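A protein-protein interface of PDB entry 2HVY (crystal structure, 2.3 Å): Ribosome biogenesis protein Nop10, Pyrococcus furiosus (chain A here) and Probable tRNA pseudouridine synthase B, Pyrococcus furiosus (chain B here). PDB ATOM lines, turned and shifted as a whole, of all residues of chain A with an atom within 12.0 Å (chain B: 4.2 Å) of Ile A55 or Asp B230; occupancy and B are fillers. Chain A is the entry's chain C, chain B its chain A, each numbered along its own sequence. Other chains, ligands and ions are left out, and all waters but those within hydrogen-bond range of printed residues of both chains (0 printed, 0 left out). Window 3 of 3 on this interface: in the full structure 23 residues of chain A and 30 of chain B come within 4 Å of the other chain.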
ATOM      1  N   GLY A  42      -9.990  23.686 -16.731  1.00  0.00           N
ATOM      2  CA  GLY A  42     -10.434  24.127 -15.407  1.00  0.00           C
ATOM      3  C   GLY A  42     -11.903  24.503 -15.329  1.00  0.00           C
ATOM      4  O   GLY A  42     -12.543  24.297 -14.296  1.00  0.00           O
ATOM      5  N   GLU A  43     -12.434  25.052 -16.421  1.00  0.00           N
ATOM      6  CA  GLU A  43     -13.849  25.422 -16.505  1.00  0.00           C
ATOM      7  C   GLU A  43     -14.765  24.201 -16.446  1.00  0.00           C
ATOM      8  O   GLU A  43     -15.840  24.252 -15.847  1.00  0.00           O
ATOM      9  CB  GLU A  43     -14.127  26.224 -17.781  1.00  0.00           C
ATOM     10  CG  GLU A  43     -13.661  27.678 -17.727  1.00  0.00           C
ATOM     11  CD  GLU A  43     -14.426  28.515 -16.709  1.00  0.00           C
ATOM     12  OE1 GLU A  43     -15.663  28.357 -16.603  1.00  0.00           O
ATOM     13  OE2 GLU A  43     -13.785  29.339 -16.023  1.00  0.00           O
ATOM     14  N   ARG A  45     -13.804  21.207 -15.128  1.00  0.00           N
ATOM     15  CA  ARG A  45     -13.599  20.680 -13.779  1.00  0.00           C
ATOM     16  C   ARG A  45     -14.503  21.398 -12.767  1.00  0.00           C
ATOM     17  O   ARG A  45     -15.059  20.765 -11.866  1.00  0.00           O
ATOM     18  CB  ARG A  45     -12.125  20.806 -13.369  1.00  0.00           C
ATOM     19  CG  ARG A  45     -11.760  20.064 -12.087  1.00  0.00           C
ATOM     20  CD  ARG A  45     -10.294  20.250 -11.701  1.00  0.00           C
ATOM     21  NE  ARG A  45      -9.973  21.630 -11.330  1.00  0.00           N
ATOM     22  CZ  ARG A  45      -9.144  22.422 -12.009  1.00  0.00           C
ATOM     23  NH1 ARG A  45      -8.530  21.978 -13.094  1.00  0.00           N
ATOM     24  NH2 ARG A  45      -8.917  23.661 -11.592  1.00  0.00           N
ATOM     25  N   ARG A  46     -14.651  22.713 -12.933  1.00  0.00           N
ATOM     26  CA  ARG A  46     -15.502  23.527 -12.059  1.00  0.00           C
ATOM     27  C   ARG A  46     -16.992  23.206 -12.165  1.00  0.00           C
ATOM     28  O   ARG A  46     -17.713  23.303 -11.174  1.00  0.00           O
ATOM     29  CB  ARG A  46     -15.273  25.018 -12.307  1.00  0.00           C
ATOM     30  CG  ARG A  46     -14.100  25.573 -11.538  1.00  0.00           C
ATOM     31  CD  ARG A  46     -13.763  26.987 -11.952  1.00  0.00           C
ATOM     32  NE  ARG A  46     -12.315  27.139 -11.996  1.00  0.00           N
ATOM     33  CZ  ARG A  46     -11.611  27.399 -13.093  1.00  0.00           C
ATOM     34  NH1 ARG A  46     -12.217  27.588 -14.257  1.00  0.00           N
ATOM     35  NH2 ARG A  46     -10.292  27.498 -13.012  1.00  0.00           N
ATOM     36  N   ARG A  47     -17.444  22.839 -13.363  1.00  0.00           N
ATOM     37  CA  ARG A  47     -18.834  22.428 -13.576  1.00  0.00           C
ATOM     38  C   ARG A  47     -19.143  21.166 -12.775  1.00  0.00           C
ATOM     39  O   ARG A  47     -20.188  21.068 -12.129  1.00  0.00           O
ATOM     40  CB  ARG A  47     -19.115  22.203 -15.065  1.00  0.00           C
ATOM     41  CG  ARG A  47     -19.130  23.478 -15.890  1.00  0.00           C
ATOM     42  CD  ARG A  47     -19.557  23.221 -17.327  1.00  0.00           C
ATOM     43  NE  ARG A  47     -19.367  24.407 -18.160  1.00  0.00           N
ATOM     44  CZ  ARG A  47     -19.580  24.454 -19.472  1.00  0.00           C
ATOM     45  NH1 ARG A  47     -19.999  23.377 -20.127  1.00  0.00           N
ATOM     46  NH2 ARG A  47     -19.377  25.587 -20.132  1.00  0.00           N
ATOM     47  N   TRP A  48     -18.215  20.213 -12.823  1.00  0.00           N
ATOM     48  CA  TRP A  48     -18.263  19.007 -12.004  1.00  0.00           C
ATOM     49  C   TRP A  48     -18.202  19.339 -10.510  1.00  0.00           C
ATOM     50  O   TRP A  48     -18.970  18.790  -9.719  1.00  0.00           O
ATOM     51  CB  TRP A  48     -17.117  18.069 -12.403  1.00  0.00           C
ATOM     52  CG  TRP A  48     -16.724  17.047 -11.371  1.00  0.00           C
ATOM     53  CD1 TRP A  48     -17.458  15.970 -10.959  1.00  0.00           C
ATOM     54  CD2 TRP A  48     -15.490  16.995 -10.642  1.00  0.00           C
ATOM     55  NE1 TRP A  48     -16.762  15.258 -10.011  1.00  0.00           N
ATOM     56  CE2 TRP A  48     -15.551  15.864  -9.797  1.00  0.00           C
ATOM     57  CE3 TRP A  48     -14.342  17.800 -10.614  1.00  0.00           C
ATOM     58  CZ2 TRP A  48     -14.506  15.514  -8.935  1.00  0.00           C
ATOM     59  CZ3 TRP A  48     -13.301  17.450  -9.755  1.00  0.00           C
ATOM     60  CH2 TRP A  48     -13.393  16.316  -8.927  1.00  0.00           C
ATOM     61  N   LYS A  49     -17.299  20.248 -10.142  1.00  0.00           N
ATOM     62  CA  LYS A  49     -17.083  20.622  -8.743  1.00  0.00           C
ATOM     63  C   LYS A  49     -18.265  21.401  -8.154  1.00  0.00           C
ATOM     64  O   LYS A  49     -18.622  21.196  -6.994  1.00  0.00           O
ATOM     65  CB  LYS A  49     -15.774  21.407  -8.588  1.00  0.00           C
ATOM     66  CG  LYS A  49     -15.230  21.450  -7.158  1.00  0.00           C
ATOM     67  CD  LYS A  49     -13.761  21.870  -7.110  1.00  0.00           C
ATOM     68  CE  LYS A  49     -12.829  20.739  -7.545  1.00  0.00           C
ATOM     69  NZ  LYS A  49     -11.393  21.153  -7.511  1.00  0.00           N
ATOM     70  N   ARG A  50     -18.863  22.284  -8.953  1.00  0.00           N
ATOM     71  CA  ARG A  50     -20.063  23.020  -8.542  1.00  0.00           C
ATOM     72  C   ARG A  50     -21.257  22.090  -8.345  1.00  0.00           C
ATOM     73  O   ARG A  50     -22.092  22.323  -7.470  1.00  0.00           O
ATOM     74  CB  ARG A  50     -20.415  24.116  -9.554  1.00  0.00           C
ATOM     75  CG  ARG A  50     -19.575  25.378  -9.427  1.00  0.00           C
ATOM     76  CD  ARG A  50     -20.032  26.446 -10.405  1.00  0.00           C
ATOM     77  NE  ARG A  50     -19.269  27.683 -10.265  1.00  0.00           N
ATOM     78  CZ  ARG A  50     -18.270  28.055 -11.063  1.00  0.00           C
ATOM     79  NH1 ARG A  50     -17.896  27.289 -12.081  1.00  0.00           N
ATOM     80  NH2 ARG A  50     -17.641  29.203 -10.843  1.00  0.00           N
ATOM     81  N   GLU A  51     -21.328  21.043  -9.166  1.00  0.00           N
ATOM     82  CA  GLU A  51     -22.353  20.007  -9.049  1.00  0.00           C
ATOM     83  C   GLU A  51     -22.204  19.236  -7.733  1.00  0.00           C
ATOM     84  O   GLU A  51     -23.188  19.002  -7.029  1.00  0.00           O
ATOM     85  CB  GLU A  51     -22.278  19.052 -10.247  1.00  0.00           C
ATOM     86  CG  GLU A  51     -23.280  17.899 -10.223  1.00  0.00           C
ATOM     87  CD  GLU A  51     -22.830  16.704 -11.052  1.00  0.00           C
ATOM     88  OE1 GLU A  51     -21.612  16.420 -11.094  1.00  0.00           O
ATOM     89  OE2 GLU A  51     -23.699  16.040 -11.656  1.00  0.00           O
ATOM     90  N   VAL A  52     -20.966  18.856  -7.413  1.00  0.00           N
ATOM     91  CA  VAL A  52     -20.658  18.094  -6.200  1.00  0.00           C
ATOM     92  C   VAL A  52     -20.923  18.918  -4.934  1.00  0.00           C
ATOM     93  O   VAL A  52     -21.606  18.452  -4.017  1.00  0.00           O
ATOM     94  CB  VAL A  52     -19.194  17.551  -6.216  1.00  0.00           C
ATOM     95  CG1 VAL A  52     -18.811  16.935  -4.873  1.00  0.00           C
ATOM     96  CG2 VAL A  52     -19.012  16.529  -7.334  1.00  0.00           C
ATOM     97  N   LEU A  53     -20.399  20.143  -4.906  1.00  0.00           N
ATOM     98  CA  LEU A  53     -20.534  21.027  -3.743  1.00  0.00           C
ATOM     99  C   LEU A  53     -21.927  21.654  -3.609  1.00  0.00           C
ATOM    100  O   LEU A  53     -22.276  22.179  -2.550  1.00  0.00           O
ATOM    101  CB  LEU A  53     -19.458  22.124  -3.765  1.00  0.00           C
ATOM    102  CG  LEU A  53     -17.980  21.710  -3.767  1.00  0.00           C
ATOM    103  CD1 LEU A  53     -17.085  22.933  -3.906  1.00  0.00           C
ATOM    104  CD2 LEU A  53     -17.605  20.903  -2.525  1.00  0.00           C
ATOM    105  N   GLY A  54     -22.714  21.593  -4.682  1.00  0.00           N
ATOM    106  CA  GLY A  54     -24.062  22.156  -4.694  1.00  0.00           C
ATOM    107  C   GLY A  54     -24.069  23.661  -4.880  1.00  0.00           C
ATOM    108  O   GLY A  54     -24.718  24.384  -4.121  1.00  0.00           O
ATOM    109  N   ILE A  55     -23.346  24.127  -5.895  1.00  0.00           N
ATOM    110  CA  ILE A  55     -23.246  25.551  -6.208  1.00  0.00           C
ATOM    111  C   ILE A  55     -23.904  25.840  -7.556  1.00  0.00           C
ATOM    112  O   ILE A  55     -25.016  26.366  -7.614  1.00  0.00           O
ATOM    113  CB  ILE A  55     -21.770  26.034  -6.217  1.00  0.00           C
ATOM    114  CG1 ILE A  55     -21.125  25.817  -4.842  1.00  0.00           C
ATOM    115  CG2 ILE A  55     -21.682  27.507  -6.629  1.00  0.00           C
ATOM    116  CD1 ILE A  55     -19.602  25.836  -4.844  1.00  0.00           C
ATOM    117  N   TYR B 225     -12.019  30.914  -7.781  1.00  0.00           N
ATOM    118  CA  TYR B 225     -13.034  31.160  -8.809  1.00  0.00           C
ATOM    119  C   TYR B 225     -14.454  31.228  -8.246  1.00  0.00           C
ATOM    120  O   TYR B 225     -15.265  32.022  -8.722  1.00  0.00           O
ATOM    121  CB  TYR B 225     -12.955  30.109  -9.920  1.00  0.00           C
ATOM    122  CG  TYR B 225     -12.040  30.488 -11.064  1.00  0.00           C
ATOM    123  CD1 TYR B 225     -10.659  30.310 -10.968  1.00  0.00           C
ATOM    124  CD2 TYR B 225     -12.555  31.021 -12.244  1.00  0.00           C
ATOM    125  CE1 TYR B 225      -9.814  30.656 -12.017  1.00  0.00           C
ATOM    126  CE2 TYR B 225     -11.718  31.369 -13.302  1.00  0.00           C
ATOM    127  CZ  TYR B 225     -10.349  31.182 -13.179  1.00  0.00           C
ATOM    128  OH  TYR B 225      -9.516  31.525 -14.216  1.00  0.00           O
ATOM    129  N   PHE B 226     -14.746  30.407  -7.237  1.00  0.00           N
ATOM    130  CA  PHE B 226     -16.047  30.448  -6.557  1.00  0.00           C
ATOM    131  C   PHE B 226     -16.244  31.771  -5.812  1.00  0.00           C
ATOM    132  O   PHE B 226     -17.375  32.201  -5.589  1.00  0.00           O
ATOM    133  CB  PHE B 226     -16.220  29.272  -5.581  1.00  0.00           C
ATOM    134  CG  PHE B 226     -16.125  27.907  -6.222  1.00  0.00           C
ATOM    135  CD1 PHE B 226     -15.666  26.820  -5.483  1.00  0.00           C
ATOM    136  CD2 PHE B 226     -16.489  27.703  -7.551  1.00  0.00           C
ATOM    137  CE1 PHE B 226     -15.572  25.553  -6.055  1.00  0.00           C
ATOM    138  CE2 PHE B 226     -16.395  26.441  -8.131  1.00  0.00           C
ATOM    139  CZ  PHE B 226     -15.936  25.365  -7.382  1.00  0.00           C
ATOM    140  N   LYS B 228     -14.517  34.847  -6.833  1.00  0.00           N
ATOM    141  CA  LYS B 228     -14.523  35.906  -7.846  1.00  0.00           C
ATOM    142  C   LYS B 228     -15.763  35.946  -8.737  1.00  0.00           C
ATOM    143  O   LYS B 228     -16.205  37.024  -9.139  1.00  0.00           O
ATOM    144  CB  LYS B 228     -13.258  35.830  -8.708  1.00  0.00           C
ATOM    145  CG  LYS B 228     -12.228  36.916  -8.412  1.00  0.00           C
ATOM    146  CD  LYS B 228     -11.639  36.793  -7.017  1.00  0.00           C
ATOM    147  CE  LYS B 228     -10.822  38.026  -6.653  1.00  0.00           C
ATOM    148  NZ  LYS B 228     -11.673  39.172  -6.221  1.00  0.00           N
ATOM    149  N   GLU B 229     -16.317  34.776  -9.046  1.00  0.00           N
ATOM    150  CA  GLU B 229     -17.443  34.677  -9.975  1.00  0.00           C
ATOM    151  C   GLU B 229     -18.788  34.473  -9.283  1.00  0.00           C
ATOM    152  O   GLU B 229     -19.793  35.060  -9.691  1.00  0.00           O
ATOM    153  CB  GLU B 229     -17.209  33.554 -10.991  1.00  0.00           C
ATOM    154  CG  GLU B 229     -15.997  33.761 -11.891  1.00  0.00           C
ATOM    155  CD  GLU B 229     -15.772  32.611 -12.852  1.00  0.00           C
ATOM    156  OE1 GLU B 229     -15.460  32.881 -14.031  1.00  0.00           O
ATOM    157  OE2 GLU B 229     -15.910  31.440 -12.438  1.00  0.00           O
ATOM    158  N   ASP B 230     -18.803  33.642  -8.245  1.00  0.00           N
ATOM    159  CA  ASP B 230     -20.045  33.277  -7.561  1.00  0.00           C
ATOM    160  C   ASP B 230     -20.307  34.099  -6.295  1.00  0.00           C
ATOM    161  O   ASP B 230     -21.413  34.069  -5.752  1.00  0.00           O
ATOM    162  CB  ASP B 230     -20.059  31.776  -7.238  1.00  0.00           C
ATOM    163  CG  ASP B 230     -19.748  30.906  -8.448  1.00  0.00           C
ATOM    164  OD1 ASP B 230     -19.145  29.828  -8.262  1.00  0.00           O
ATOM    165  OD2 ASP B 230     -20.101  31.293  -9.584  1.00  0.00           O
ATOM    166  N   GLY B 231     -19.292  34.828  -5.833  1.00  0.00           N
ATOM    167  CA  GLY B 231     -19.404  35.651  -4.623  1.00  0.00           C
ATOM    168  C   GLY B 231     -19.302  34.866  -3.324  1.00  0.00           C
ATOM    169  O   GLY B 231     -19.474  35.426  -2.239  1.00  0.00           O
ATOM    170  N   ILE B 232     -19.015  33.571  -3.445  1.00  0.00           N
ATOM    171  CA  ILE B 232     -18.899  32.663  -2.307  1.00  0.00           C
ATOM    172  C   ILE B 232     -17.484  32.733  -1.734  1.00  0.00           C
ATOM    173  O   ILE B 232     -16.539  32.221  -2.336  1.00  0.00           O
ATOM    174  CB  ILE B 232     -19.212  31.191  -2.728  1.00  0.00           C
ATOM    175  CG1 ILE B 232     -20.534  31.087  -3.515  1.00  0.00           C
ATOM    176  CG2 ILE B 232     -19.182  30.246  -1.525  1.00  0.00           C
ATOM    177  CD1 ILE B 232     -21.792  31.503  -2.746  1.00  0.00           C
ATOM    178  N   TYR B 235     -15.275  29.108   0.897  1.00  0.00           N
ATOM    179  CA  TYR B 235     -14.320  28.093   0.441  1.00  0.00           C
ATOM    180  C   TYR B 235     -12.891  28.637   0.334  1.00  0.00           C
ATOM    181  O   TYR B 235     -11.942  27.978   0.763  1.00  0.00           O
ATOM    182  CB  TYR B 235     -14.759  27.476  -0.892  1.00  0.00           C
ATOM    183  CG  TYR B 235     -16.029  26.655  -0.818  1.00  0.00           C
ATOM    184  CD1 TYR B 235     -17.229  27.145  -1.331  1.00  0.00           C
ATOM    185  CD2 TYR B 235     -16.031  25.385  -0.241  1.00  0.00           C
ATOM    186  CE1 TYR B 235     -18.400  26.396  -1.267  1.00  0.00           C
ATOM    187  CE2 TYR B 235     -17.198  24.625  -0.172  1.00  0.00           C
ATOM    188  CZ  TYR B 235     -18.377  25.138  -0.688  1.00  0.00           C
ATOM    189  OH  TYR B 235     -19.532  24.391  -0.625  1.00  0.00           O
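The guanidinium group (NE) of Arg A50 is in salt-bridge range of the side-chain carboxylate (OD1) of Asp B230 (2.9 Å).
The side-chain carboxylate of Glu B229 is in salt-bridge range of the guanidinium group of Arg A50 (3.2 Å).
The backbone NH (N) of Gly B231 lies within hydrogen-bond range of the backbone carbonyl oxygen (O) of Phe B226, 3.3 Å away.
The side-chain carboxylate (OE2) of Glu A43 is in salt-bridge range of the guanidinium group (NH1) of Arg A46, 2.9 Å away.
The backbone NH of Ile A55 lies within hydrogen-bond range of the backbone carbonyl oxygen of Arg A50 (2.7 Å).
The guanidinium group of Arg A46 sits close to the backbone carbonyl oxygen of Gly A42, 3.3 Å away.
The backbone NH of Ile B232 is in hydrogen-bond range of the backbone carbonyl oxygen of Phe B226.
Among the printed residues, pairs that only touch across the chains: Glu A43 with Tyr B225 (3.97 Å), Arg A46 with Tyr B225 (3.3 Å), Lys A49 with Phe B226 (3.98 Å), Arg A50 with Phe B226 (3.6 Å), Leu A53 with Phe B226 (3.7 Å), Leu A53 with Tyr B235 (3.9 Å), Ile A55 with Asp B230 (3.8 Å) and Ile A55 with Tyr B235 (3.8 Å).
Printed residues of chain B within 4 Å of Glu A43: Tyr B225.
Printed residues of chain B within 4 Å of Lys A49: Phe B226.
Ile A55 touches just these residues of chain B: Asp B230 and Tyr B235.
Of chain A, only Arg A50 comes within 4 Å of Glu B229.
Of chain A, only Arg A50 (2.9 Å) and Ile A55 (3.8 Å) come within 4 Å of Asp B230.
No residue of chain A comes within 4 Å of Gly B231.
Of the printed residues of chain A, Tyr B235 touches Leu A53 (3.9 Å) and Ile A55 (3.8 Å).
The nearest residue of chain A that does not touch Asp B230 is Arg A46 (7.1 Å).
Printed residues of chain A that touch a printed residue of chain B: Glu A43, Arg A46, Lys A49, Arg A50, Leu A53 and Ile A55.
Along chain A the printed residues that touch a printed residue of chain B span positions 43 to 55.
Of the 8 printed residues of chain B, 5 touch a printed residue of chain A.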
